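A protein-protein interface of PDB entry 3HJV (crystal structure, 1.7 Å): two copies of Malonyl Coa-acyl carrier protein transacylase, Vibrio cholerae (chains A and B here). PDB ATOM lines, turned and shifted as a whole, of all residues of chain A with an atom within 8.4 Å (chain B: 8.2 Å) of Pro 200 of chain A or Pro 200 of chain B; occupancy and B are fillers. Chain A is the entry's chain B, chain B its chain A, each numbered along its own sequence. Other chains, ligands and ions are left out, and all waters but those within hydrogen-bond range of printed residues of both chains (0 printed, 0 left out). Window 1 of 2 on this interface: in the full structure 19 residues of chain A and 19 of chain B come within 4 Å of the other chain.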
ATOM      1  N   GLN A  16     -11.030   8.366  15.436  1.00  0.00           N
ATOM      2  CA  GLN A  16     -10.607   7.275  16.289  1.00  0.00           C
ATOM      3  C   GLN A  16     -10.951   5.903  15.711  1.00  0.00           C
ATOM      4  O   GLN A  16     -12.094   5.631  15.308  1.00  0.00           O
ATOM      5  CB  GLN A  16     -11.234   7.433  17.678  1.00  0.00           C
ATOM      6  CG  GLN A  16     -10.740   6.448  18.742  1.00  0.00           C
ATOM      7  CD  GLN A  16      -9.394   6.795  19.308  1.00  0.00           C
ATOM      8  OE1 GLN A  16      -9.053   7.981  19.462  1.00  0.00           O
ATOM      9  NE2 GLN A  16      -8.622   5.762  19.681  1.00  0.00           N
ATOM     10  N   GLU A  59      -0.792  -0.080  22.406  1.00  0.00           N
ATOM     11  CA  GLU A  59      -1.702   0.256  23.492  1.00  0.00           C
ATOM     12  C   GLU A  59      -1.633   1.742  23.808  1.00  0.00           C
ATOM     13  O   GLU A  59      -2.649   2.342  24.115  1.00  0.00           O
ATOM     14  CB  GLU A  59      -1.488  -0.613  24.740  1.00  0.00           C
ATOM     15  CG  GLU A  59      -1.655  -2.116  24.511  1.00  0.00           C
ATOM     16  CD  GLU A  59      -0.360  -2.841  24.114  1.00  0.00           C
ATOM     17  OE1 GLU A  59       0.644  -2.174  23.714  1.00  0.00           O
ATOM     18  OE2 GLU A  59      -0.330  -4.091  24.274  1.00  0.00           O
ATOM     19  N   ASN A  62      -3.333   3.723  20.888  1.00  0.00           N
ATOM     20  CA  ASN A  62      -4.780   3.608  20.977  1.00  0.00           C
ATOM     21  C   ASN A  62      -5.440   4.431  22.093  1.00  0.00           C
ATOM     22  O   ASN A  62      -6.673   4.511  22.115  1.00  0.00           O
ATOM     23  CB  ASN A  62      -5.218   2.143  21.158  1.00  0.00           C
ATOM     24  CG  ASN A  62      -4.927   1.277  19.948  1.00  0.00           C
ATOM     25  OD1 ASN A  62      -4.656   1.776  18.856  1.00  0.00           O
ATOM     26  ND2 ASN A  62      -5.025  -0.025  20.131  1.00  0.00           N
ATOM     27  N   GLN A  63      -4.655   5.029  22.998  1.00  0.00           N
ATOM     28  CA  GLN A  63      -5.203   5.884  24.055  1.00  0.00           C
ATOM     29  C   GLN A  63      -5.622   7.148  23.342  1.00  0.00           C
ATOM     30  O   GLN A  63      -4.832   7.730  22.616  1.00  0.00           O
ATOM     31  CB  GLN A  63      -4.183   6.213  25.123  1.00  0.00           C
ATOM     32  CG  GLN A  63      -3.594   5.022  25.846  1.00  0.00           C
ATOM     33  CD  GLN A  63      -4.599   4.261  26.688  1.00  0.00           C
ATOM     34  OE1 GLN A  63      -4.796   3.056  26.501  1.00  0.00           O
ATOM     35  NE2 GLN A  63      -5.229   4.947  27.625  1.00  0.00           N
ATOM     36  N   THR A  64      -6.846   7.584  23.578  1.00  0.00           N
ATOM     37  CA  THR A  64      -7.393   8.663  22.783  1.00  0.00           C
ATOM     38  C   THR A  64      -6.594   9.969  22.793  1.00  0.00           C
ATOM     39  O   THR A  64      -6.574  10.663  21.782  1.00  0.00           O
ATOM     40  CB  THR A  64      -8.879   8.906  23.070  1.00  0.00           C
ATOM     41  OG1 THR A  64      -9.442   9.661  21.973  1.00  0.00           O
ATOM     42  CG2 THR A  64      -9.054   9.600  24.396  1.00  0.00           C
ATOM     43  N   GLY A 135     -20.075   4.335  31.705  1.00  0.00           N
ATOM     44  CA  GLY A 135     -20.581   4.582  30.352  1.00  0.00           C
ATOM     45  C   GLY A 135     -20.513   3.349  29.453  1.00  0.00           C
ATOM     46  O   GLY A 135     -19.822   2.380  29.753  1.00  0.00           O
ATOM     47  N   ALA A 136     -21.272   3.373  28.363  1.00  0.00           N
ATOM     48  CA  ALA A 136     -21.245   2.294  27.382  1.00  0.00           C
ATOM     49  C   ALA A 136     -21.621   2.816  26.004  1.00  0.00           C
ATOM     50  O   ALA A 136     -22.202   3.898  25.861  1.00  0.00           O
ATOM     51  CB  ALA A 136     -22.182   1.148  27.766  1.00  0.00           C
ATOM     52  N   MET A 137     -21.218   2.066  24.982  1.00  0.00           N
ATOM     53  CA  MET A 137     -21.562   2.369  23.599  1.00  0.00           C
ATOM     54  C   MET A 137     -21.975   1.056  22.932  1.00  0.00           C
ATOM     55  O   MET A 137     -21.377  -0.001  23.201  1.00  0.00           O
ATOM     56  CB  MET A 137     -20.396   3.007  22.813  1.00  0.00           C
ATOM     57  CG  MET A 137     -19.857   4.338  23.371  1.00  0.00           C
ATOM     58  SD  MET A 137     -18.680   5.333  22.111  1.00  0.00           S
ATOM     59  CE  MET A 137     -20.006   5.791  20.771  1.00  0.00           C
ATOM     60  N   TYR A 138     -23.008   1.123  22.090  1.00  0.00           N
ATOM     61  CA  TYR A 138     -23.499  -0.038  21.328  1.00  0.00           C
ATOM     62  C   TYR A 138     -23.691   0.333  19.863  1.00  0.00           C
ATOM     63  O   TYR A 138     -24.198   1.406  19.559  1.00  0.00           O
ATOM     64  CB  TYR A 138     -24.867  -0.515  21.824  1.00  0.00           C
ATOM     65  CG  TYR A 138     -24.893  -1.599  22.879  1.00  0.00           C
ATOM     66  CD1 TYR A 138     -24.172  -1.479  24.055  1.00  0.00           C
ATOM     67  CD2 TYR A 138     -25.743  -2.695  22.736  1.00  0.00           C
ATOM     68  CE1 TYR A 138     -24.230  -2.454  25.030  1.00  0.00           C
ATOM     69  CE2 TYR A 138     -25.809  -3.673  23.717  1.00  0.00           C
ATOM     70  CZ  TYR A 138     -25.051  -3.537  24.863  1.00  0.00           C
ATOM     71  OH  TYR A 138     -25.113  -4.516  25.852  1.00  0.00           O
ATOM     72  N   ALA A 139     -23.310  -0.575  18.962  1.00  0.00           N
ATOM     73  CA  ALA A 139     -23.604  -0.380  17.561  1.00  0.00           C
ATOM     74  C   ALA A 139     -24.924  -1.099  17.282  1.00  0.00           C
ATOM     75  O   ALA A 139     -25.056  -2.284  17.580  1.00  0.00           O
ATOM     76  CB  ALA A 139     -22.486  -0.939  16.670  1.00  0.00           C
ATOM     77  N   LEU A 197     -24.405  -4.550  19.087  1.00  0.00           N
ATOM     78  CA  LEU A 197     -23.057  -4.949  19.467  1.00  0.00           C
ATOM     79  C   LEU A 197     -22.491  -4.074  20.570  1.00  0.00           C
ATOM     80  O   LEU A 197     -22.384  -2.864  20.387  1.00  0.00           O
ATOM     81  CB  LEU A 197     -22.152  -4.826  18.243  1.00  0.00           C
ATOM     82  CG  LEU A 197     -22.570  -5.570  16.972  1.00  0.00           C
ATOM     83  CD1 LEU A 197     -21.615  -5.175  15.883  1.00  0.00           C
ATOM     84  CD2 LEU A 197     -22.569  -7.085  17.181  1.00  0.00           C
ATOM     85  N   PRO A 198     -22.122  -4.672  21.715  1.00  0.00           N
ATOM     86  CA  PRO A 198     -21.527  -3.831  22.747  1.00  0.00           C
ATOM     87  C   PRO A 198     -20.142  -3.476  22.289  1.00  0.00           C
ATOM     88  O   PRO A 198     -19.392  -4.366  21.880  1.00  0.00           O
ATOM     89  CB  PRO A 198     -21.506  -4.738  23.983  1.00  0.00           C
ATOM     90  CG  PRO A 198     -21.443  -6.110  23.438  1.00  0.00           C
ATOM     91  CD  PRO A 198     -22.143  -6.094  22.101  1.00  0.00           C
ATOM     92  N   LEU A 199     -19.801  -2.195  22.305  1.00  0.00           N
ATOM     93  CA  LEU A 199     -18.486  -1.775  21.856  1.00  0.00           C
ATOM     94  C   LEU A 199     -17.535  -1.641  23.032  1.00  0.00           C
ATOM     95  O   LEU A 199     -17.884  -1.057  24.055  1.00  0.00           O
ATOM     96  CB  LEU A 199     -18.555  -0.455  21.093  1.00  0.00           C
ATOM     97  CG  LEU A 199     -19.524  -0.444  19.901  1.00  0.00           C
ATOM     98  CD1 LEU A 199     -19.387   0.833  19.154  1.00  0.00           C
ATOM     99  CD2 LEU A 199     -19.276  -1.631  18.968  1.00  0.00           C
ATOM    100  N   PRO A 200     -16.314  -2.167  22.875  1.00  0.00           N
ATOM    101  CA  PRO A 200     -15.358  -2.090  23.952  1.00  0.00           C
ATOM    102  C   PRO A 200     -14.831  -0.658  24.069  1.00  0.00           C
ATOM    103  O   PRO A 200     -13.881  -0.279  23.376  1.00  0.00           O
ATOM    104  CB  PRO A 200     -14.270  -3.066  23.504  1.00  0.00           C
ATOM    105  CG  PRO A 200     -14.285  -2.979  22.010  1.00  0.00           C
ATOM    106  CD  PRO A 200     -15.681  -2.583  21.608  1.00  0.00           C
ATOM    107  N   VAL A 201     -15.491   0.140  24.908  1.00  0.00           N
ATOM    108  CA  VAL A 201     -15.090   1.527  25.143  1.00  0.00           C
ATOM    109  C   VAL A 201     -15.541   1.975  26.522  1.00  0.00           C
ATOM    110  O   VAL A 201     -16.603   1.569  26.998  1.00  0.00           O
ATOM    111  CB  VAL A 201     -15.716   2.495  24.119  1.00  0.00           C
ATOM    112  CG1 VAL A 201     -15.212   2.217  22.707  1.00  0.00           C
ATOM    113  CG2 VAL A 201     -17.206   2.398  24.180  1.00  0.00           C
ATOM    114  N   SER A 202     -14.730   2.817  27.153  1.00  0.00           N
ATOM    115  CA  SER A 202     -15.044   3.385  28.464  1.00  0.00           C
ATOM    116  C   SER A 202     -15.710   4.776  28.341  1.00  0.00           C
ATOM    117  O   SER A 202     -16.508   5.172  29.207  1.00  0.00           O
ATOM    118  CB  SER A 202     -13.764   3.492  29.296  1.00  0.00           C
ATOM    119  OG  SER A 202     -12.757   4.207  28.593  1.00  0.00           O
ATOM    120  N   VAL A 203     -15.382   5.506  27.271  1.00  0.00           N
ATOM    121  CA  VAL A 203     -15.916   6.846  27.051  1.00  0.00           C
ATOM    122  C   VAL A 203     -17.224   6.842  26.252  1.00  0.00           C
ATOM    123  O   VAL A 203     -17.238   6.444  25.085  1.00  0.00           O
ATOM    124  CB  VAL A 203     -14.881   7.729  26.322  1.00  0.00           C
ATOM    125  CG1 VAL A 203     -15.419   9.138  26.122  1.00  0.00           C
ATOM    126  CG2 VAL A 203     -13.561   7.787  27.117  1.00  0.00           C
ATOM    127  N   GLN B  16      -5.122 -10.316  17.204  1.00  0.00           N
ATOM    128  CA  GLN B  16      -6.194  -9.320  17.428  1.00  0.00           C
ATOM    129  C   GLN B  16      -5.656  -7.899  17.592  1.00  0.00           C
ATOM    130  O   GLN B  16      -4.799  -7.664  18.435  1.00  0.00           O
ATOM    131  CB  GLN B  16      -6.999  -9.722  18.683  1.00  0.00           C
ATOM    132  CG  GLN B  16      -8.237  -8.851  19.004  1.00  0.00           C
ATOM    133  CD  GLN B  16      -9.421  -9.158  18.114  1.00  0.00           C
ATOM    134  OE1 GLN B  16      -9.705 -10.332  17.814  1.00  0.00           O
ATOM    135  NE2 GLN B  16     -10.182  -8.106  17.741  1.00  0.00           N
ATOM    136  N   GLU B  59     -17.396  -2.177  13.295  1.00  0.00           N
ATOM    137  CA  GLU B  59     -17.776  -2.709  14.613  1.00  0.00           C
ATOM    138  C   GLU B  59     -17.982  -4.220  14.547  1.00  0.00           C
ATOM    139  O   GLU B  59     -17.749  -4.926  15.532  1.00  0.00           O
ATOM    140  CB  GLU B  59     -19.025  -2.017  15.153  1.00  0.00           C
ATOM    141  CG  GLU B  59     -18.874  -0.506  15.311  1.00  0.00           C
ATOM    142  CD  GLU B  59     -19.272   0.310  14.097  1.00  0.00           C
ATOM    143  OE1 GLU B  59     -19.311  -0.212  12.961  1.00  0.00           O
ATOM    144  OE2 GLU B  59     -19.546   1.513  14.311  1.00  0.00           O
ATOM    145  N   ASN B  62     -14.436  -5.904  14.250  1.00  0.00           N
ATOM    146  CA  ASN B  62     -13.703  -5.868  15.532  1.00  0.00           C
ATOM    147  C   ASN B  62     -14.191  -6.892  16.576  1.00  0.00           C
ATOM    148  O   ASN B  62     -13.548  -7.061  17.623  1.00  0.00           O
ATOM    149  CB  ASN B  62     -13.731  -4.471  16.135  1.00  0.00           C
ATOM    150  CG  ASN B  62     -12.873  -3.457  15.381  1.00  0.00           C
ATOM    151  OD1 ASN B  62     -12.016  -3.803  14.554  1.00  0.00           O
ATOM    152  ND2 ASN B  62     -13.101  -2.188  15.677  1.00  0.00           N
ATOM    153  N   GLN B  63     -15.328  -7.536  16.326  1.00  0.00           N
ATOM    154  CA  GLN B  63     -15.835  -8.580  17.228  1.00  0.00           C
ATOM    155  C   GLN B  63     -14.930  -9.776  16.999  1.00  0.00           C
ATOM    156  O   GLN B  63     -14.841 -10.255  15.874  1.00  0.00           O
ATOM    157  CB  GLN B  63     -17.285  -8.938  16.922  1.00  0.00           C
ATOM    158  CG  GLN B  63     -18.277  -7.774  17.042  1.00  0.00           C
ATOM    159  CD  GLN B  63     -18.264  -7.121  18.395  1.00  0.00           C
ATOM    160  OE1 GLN B  63     -18.223  -5.893  18.498  1.00  0.00           O
ATOM    161  NE2 GLN B  63     -18.278  -7.929  19.448  1.00  0.00           N
ATOM    162  N   ALA B 136     -11.261  -7.619  33.117  1.00  0.00           N
ATOM    163  CA  ALA B 136     -10.547  -6.444  32.662  1.00  0.00           C
ATOM    164  C   ALA B 136      -9.141  -6.834  32.199  1.00  0.00           C
ATOM    165  O   ALA B 136      -8.696  -7.926  32.465  1.00  0.00           O
ATOM    166  CB  ALA B 136     -10.499  -5.366  33.758  1.00  0.00           C
ATOM    167  N   MET B 137      -8.478  -5.887  31.567  1.00  0.00           N
ATOM    168  CA  MET B 137      -7.149  -6.085  31.049  1.00  0.00           C
ATOM    169  C   MET B 137      -6.408  -4.742  31.099  1.00  0.00           C
ATOM    170  O   MET B 137      -6.990  -3.685  30.844  1.00  0.00           O
ATOM    171  CB  MET B 137      -7.243  -6.615  29.617  1.00  0.00           C
ATOM    172  CG  MET B 137      -5.948  -6.685  28.876  1.00  0.00           C
ATOM    173  SD  MET B 137      -6.101  -7.460  27.104  1.00  0.00           S
ATOM    174  CE  MET B 137      -6.504  -9.281  27.722  1.00  0.00           C
ATOM    175  N   TYR B 138      -5.131  -4.791  31.470  1.00  0.00           N
ATOM    176  CA  TYR B 138      -4.266  -3.597  31.533  1.00  0.00           C
ATOM    177  C   TYR B 138      -2.918  -3.876  30.874  1.00  0.00           C
ATOM    178  O   TYR B 138      -2.387  -4.958  31.033  1.00  0.00           O
ATOM    179  CB  TYR B 138      -3.957  -3.269  32.998  1.00  0.00           C
ATOM    180  CG  TYR B 138      -4.893  -2.337  33.722  1.00  0.00           C
ATOM    181  CD1 TYR B 138      -6.254  -2.596  33.817  1.00  0.00           C
ATOM    182  CD2 TYR B 138      -4.375  -1.249  34.425  1.00  0.00           C
ATOM    183  CE1 TYR B 138      -7.100  -1.732  34.519  1.00  0.00           C
ATOM    184  CE2 TYR B 138      -5.204  -0.398  35.140  1.00  0.00           C
ATOM    185  CZ  TYR B 138      -6.558  -0.654  35.196  1.00  0.00           C
ATOM    186  OH  TYR B 138      -7.372   0.217  35.909  1.00  0.00           O
ATOM    187  N   LEU B 197      -2.025   1.028  31.676  1.00  0.00           N
ATOM    188  CA  LEU B 197      -3.091   1.464  30.786  1.00  0.00           C
ATOM    189  C   LEU B 197      -4.268   0.510  30.800  1.00  0.00           C
ATOM    190  O   LEU B 197      -4.115  -0.656  30.418  1.00  0.00           O
ATOM    191  CB  LEU B 197      -2.554   1.549  29.353  1.00  0.00           C
ATOM    192  CG  LEU B 197      -1.220   2.284  29.118  1.00  0.00           C
ATOM    193  CD1 LEU B 197      -0.812   2.124  27.670  1.00  0.00           C
ATOM    194  CD2 LEU B 197      -1.290   3.750  29.510  1.00  0.00           C
ATOM    195  N   PRO B 198      -5.455   0.987  31.235  1.00  0.00           N
ATOM    196  CA  PRO B 198      -6.624   0.112  31.143  1.00  0.00           C
ATOM    197  C   PRO B 198      -6.987  -0.031  29.663  1.00  0.00           C
ATOM    198  O   PRO B 198      -7.027   0.972  28.940  1.00  0.00           O
ATOM    199  CB  PRO B 198      -7.716   0.867  31.944  1.00  0.00           C
ATOM    200  CG  PRO B 198      -6.986   1.965  32.664  1.00  0.00           C
ATOM    201  CD  PRO B 198      -5.792   2.290  31.820  1.00  0.00           C
ATOM    202  N   LEU B 199      -7.200  -1.266  29.207  1.00  0.00           N
ATOM    203  CA  LEU B 199      -7.521  -1.532  27.820  1.00  0.00           C
ATOM    204  C   LEU B 199      -9.025  -1.733  27.618  1.00  0.00           C
ATOM    205  O   LEU B 199      -9.678  -2.382  28.423  1.00  0.00           O
ATOM    206  CB  LEU B 199      -6.752  -2.766  27.322  1.00  0.00           C
ATOM    207  CG  LEU B 199      -5.235  -2.723  27.524  1.00  0.00           C
ATOM    208  CD1 LEU B 199      -4.571  -3.936  26.891  1.00  0.00           C
ATOM    209  CD2 LEU B 199      -4.589  -1.444  26.987  1.00  0.00           C
ATOM    210  N   PRO B 200      -9.566  -1.181  26.532  1.00  0.00           N
ATOM    211  CA  PRO B 200     -10.972  -1.330  26.185  1.00  0.00           C
ATOM    212  C   PRO B 200     -11.206  -2.736  25.651  1.00  0.00           C
ATOM    213  O   PRO B 200     -11.213  -2.958  24.446  1.00  0.00           O
ATOM    214  CB  PRO B 200     -11.165  -0.285  25.092  1.00  0.00           C
ATOM    215  CG  PRO B 200      -9.846  -0.188  24.420  1.00  0.00           C
ATOM    216  CD  PRO B 200      -8.805  -0.502  25.465  1.00  0.00           C
ATOM    217  N   VAL B 201     -11.363  -3.682  26.559  1.00  0.00           N
ATOM    218  CA  VAL B 201     -11.546  -5.079  26.200  1.00  0.00           C
ATOM    219  C   VAL B 201     -12.458  -5.705  27.235  1.00  0.00           C
ATOM    220  O   VAL B 201     -12.299  -5.471  28.437  1.00  0.00           O
ATOM    221  CB  VAL B 201     -10.199  -5.831  26.247  1.00  0.00           C
ATOM    222  CG1 VAL B 201      -9.181  -5.229  25.258  1.00  0.00           C
ATOM    223  CG2 VAL B 201      -9.659  -5.762  27.623  1.00  0.00           C
ATOM    224  N   SER B 202     -13.416  -6.486  26.776  1.00  0.00           N
ATOM    225  CA  SER B 202     -14.320  -7.187  27.678  1.00  0.00           C
ATOM    226  C   SER B 202     -13.765  -8.559  28.108  1.00  0.00           C
ATOM    227  O   SER B 202     -13.909  -8.957  29.285  1.00  0.00           O
ATOM    228  CB  SER B 202     -15.677  -7.355  26.994  1.00  0.00           C
ATOM    229  OG  SER B 202     -15.512  -7.850  25.665  1.00  0.00           O
ATOM    230  N   VAL B 203     -13.121  -9.266  27.169  1.00  0.00           N
ATOM    231  CA  VAL B 203     -12.652 -10.626  27.416  1.00  0.00           C
ATOM    232  C   VAL B 203     -11.281 -10.654  28.078  1.00  0.00           C
ATOM    233  O   VAL B 203     -10.340 -10.157  27.491  1.00  0.00           O
ATOM    234  CB  VAL B 203     -12.556 -11.417  26.087  1.00  0.00           C
ATOM    235  CG1 VAL B 203     -12.009 -12.798  26.344  1.00  0.00           C
ATOM    236  CG2 VAL B 203     -13.944 -11.521  25.389  1.00  0.00           C
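Glu 59 of chain A touches Leu 197 of chain B, and with the chains exchanged Leu 197 of chain A touches Glu 59 of chain B.
Glu 59 of chain A touches Leu 199 of chain B, and with the chains exchanged Leu 199 of chain A touches Glu 59 of chain B.
Gln 63 of chain A touches Leu 197 of chain B, but with the chains exchanged Leu 197 of chain A does not touch Gln 63 of chain B (4.1 Å).
Pro 200 of chain A touches its own counterpart, Pro 200 of chain B.
14 positions are printed for both chains.
Among the printed residues, merely in contact across the chains: Pro 200 of chain A with Pro 200 of chain B (3.2 Å), Leu 199 of chain A with Glu 59 of chain B (3.8 Å), Ala 139 of chain A with Glu 59 of chain B (3.9 Å), Leu 197 of chain A with Glu 59 of chain B (3.9 Å), Pro 198 of chain A with Gln 63 of chain B (3.9 Å), Glu 59 of chain A with Leu 199 of chain B (3.9 Å), Gln 63 of chain A with Pro 198 of chain B (3.9 Å), Gln 63 of chain A with Leu 197 of chain B (3.9 Å) and Glu 59 of chain A with Leu 197 of chain B (3.97 Å).
Hydrophobic or aromatic side chains of chain A within 4 Å of the printed part of chain B: Ala 139, Leu 197, Leu 199 and Pro 200.
Printed residues of chain B that touch a printed residue of chain A: Glu 59, Gln 63, Leu 197, Pro 198, Leu 199 and Pro 200.
Among the printed residues, no Asp or Glu carboxylate lies within 4 Å of a Lys or Arg side-chain nitrogen of the other chain.
The backbone carbonyl oxygen (O) of Ala 139 of chain A sits at hydrogen-bond distance from the backbone NH (N) of Leu 197 of chain A (2.8 Å).
O of Glu 59 of chain A sits close to OE1 of Gln 63 of chain A, at 3.3 Å.
The backbone NH of Leu 199 of chain A lies within hydrogen-bond range of the backbone carbonyl oxygen of Met 137 of chain A.
The backbone carbonyl oxygen (O) of Glu 59 of chain B lies close to the side-chain amide oxygen (OE1) of Gln 63 of chain B (3.2 Å).
The backbone NH of Leu 199 of chain B sits at hydrogen-bond distance from the backbone carbonyl oxygen of Met 137 of chain B, 2.9 Å away.
Of chain B, only Pro 200 comes within 4 Å of Pro 200 of chain A.
Pro 200 of chain B touches one residue of chain A.
No residue of chain B comes within 4 Å of Val 201 of chain A.
No residue of chain A comes within 4 Å of Val 201 of chain B.
Of the printed residues of chain B, Ala 139 of chain A touches Glu 59.
Of the printed residues of chain B, Pro 198 of chain A touches Gln 63 (3.9 Å).
Ala 136 of chain A touches none of the printed residues of chain B.
Thr 64 of chain A touches none of the printed residues of chain B.
The nearest residue of chain B that does not touch Pro 200 of chain A is Val 201 of chain B (4.3 Å).
The nearest residue of chain A that does not touch Pro 200 of chain B is Val 201 of chain A (4.3 Å).
The nearest printed residue of chain A that does not touch Glu 59 of chain B is Pro 198 of chain A (6.6 Å).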
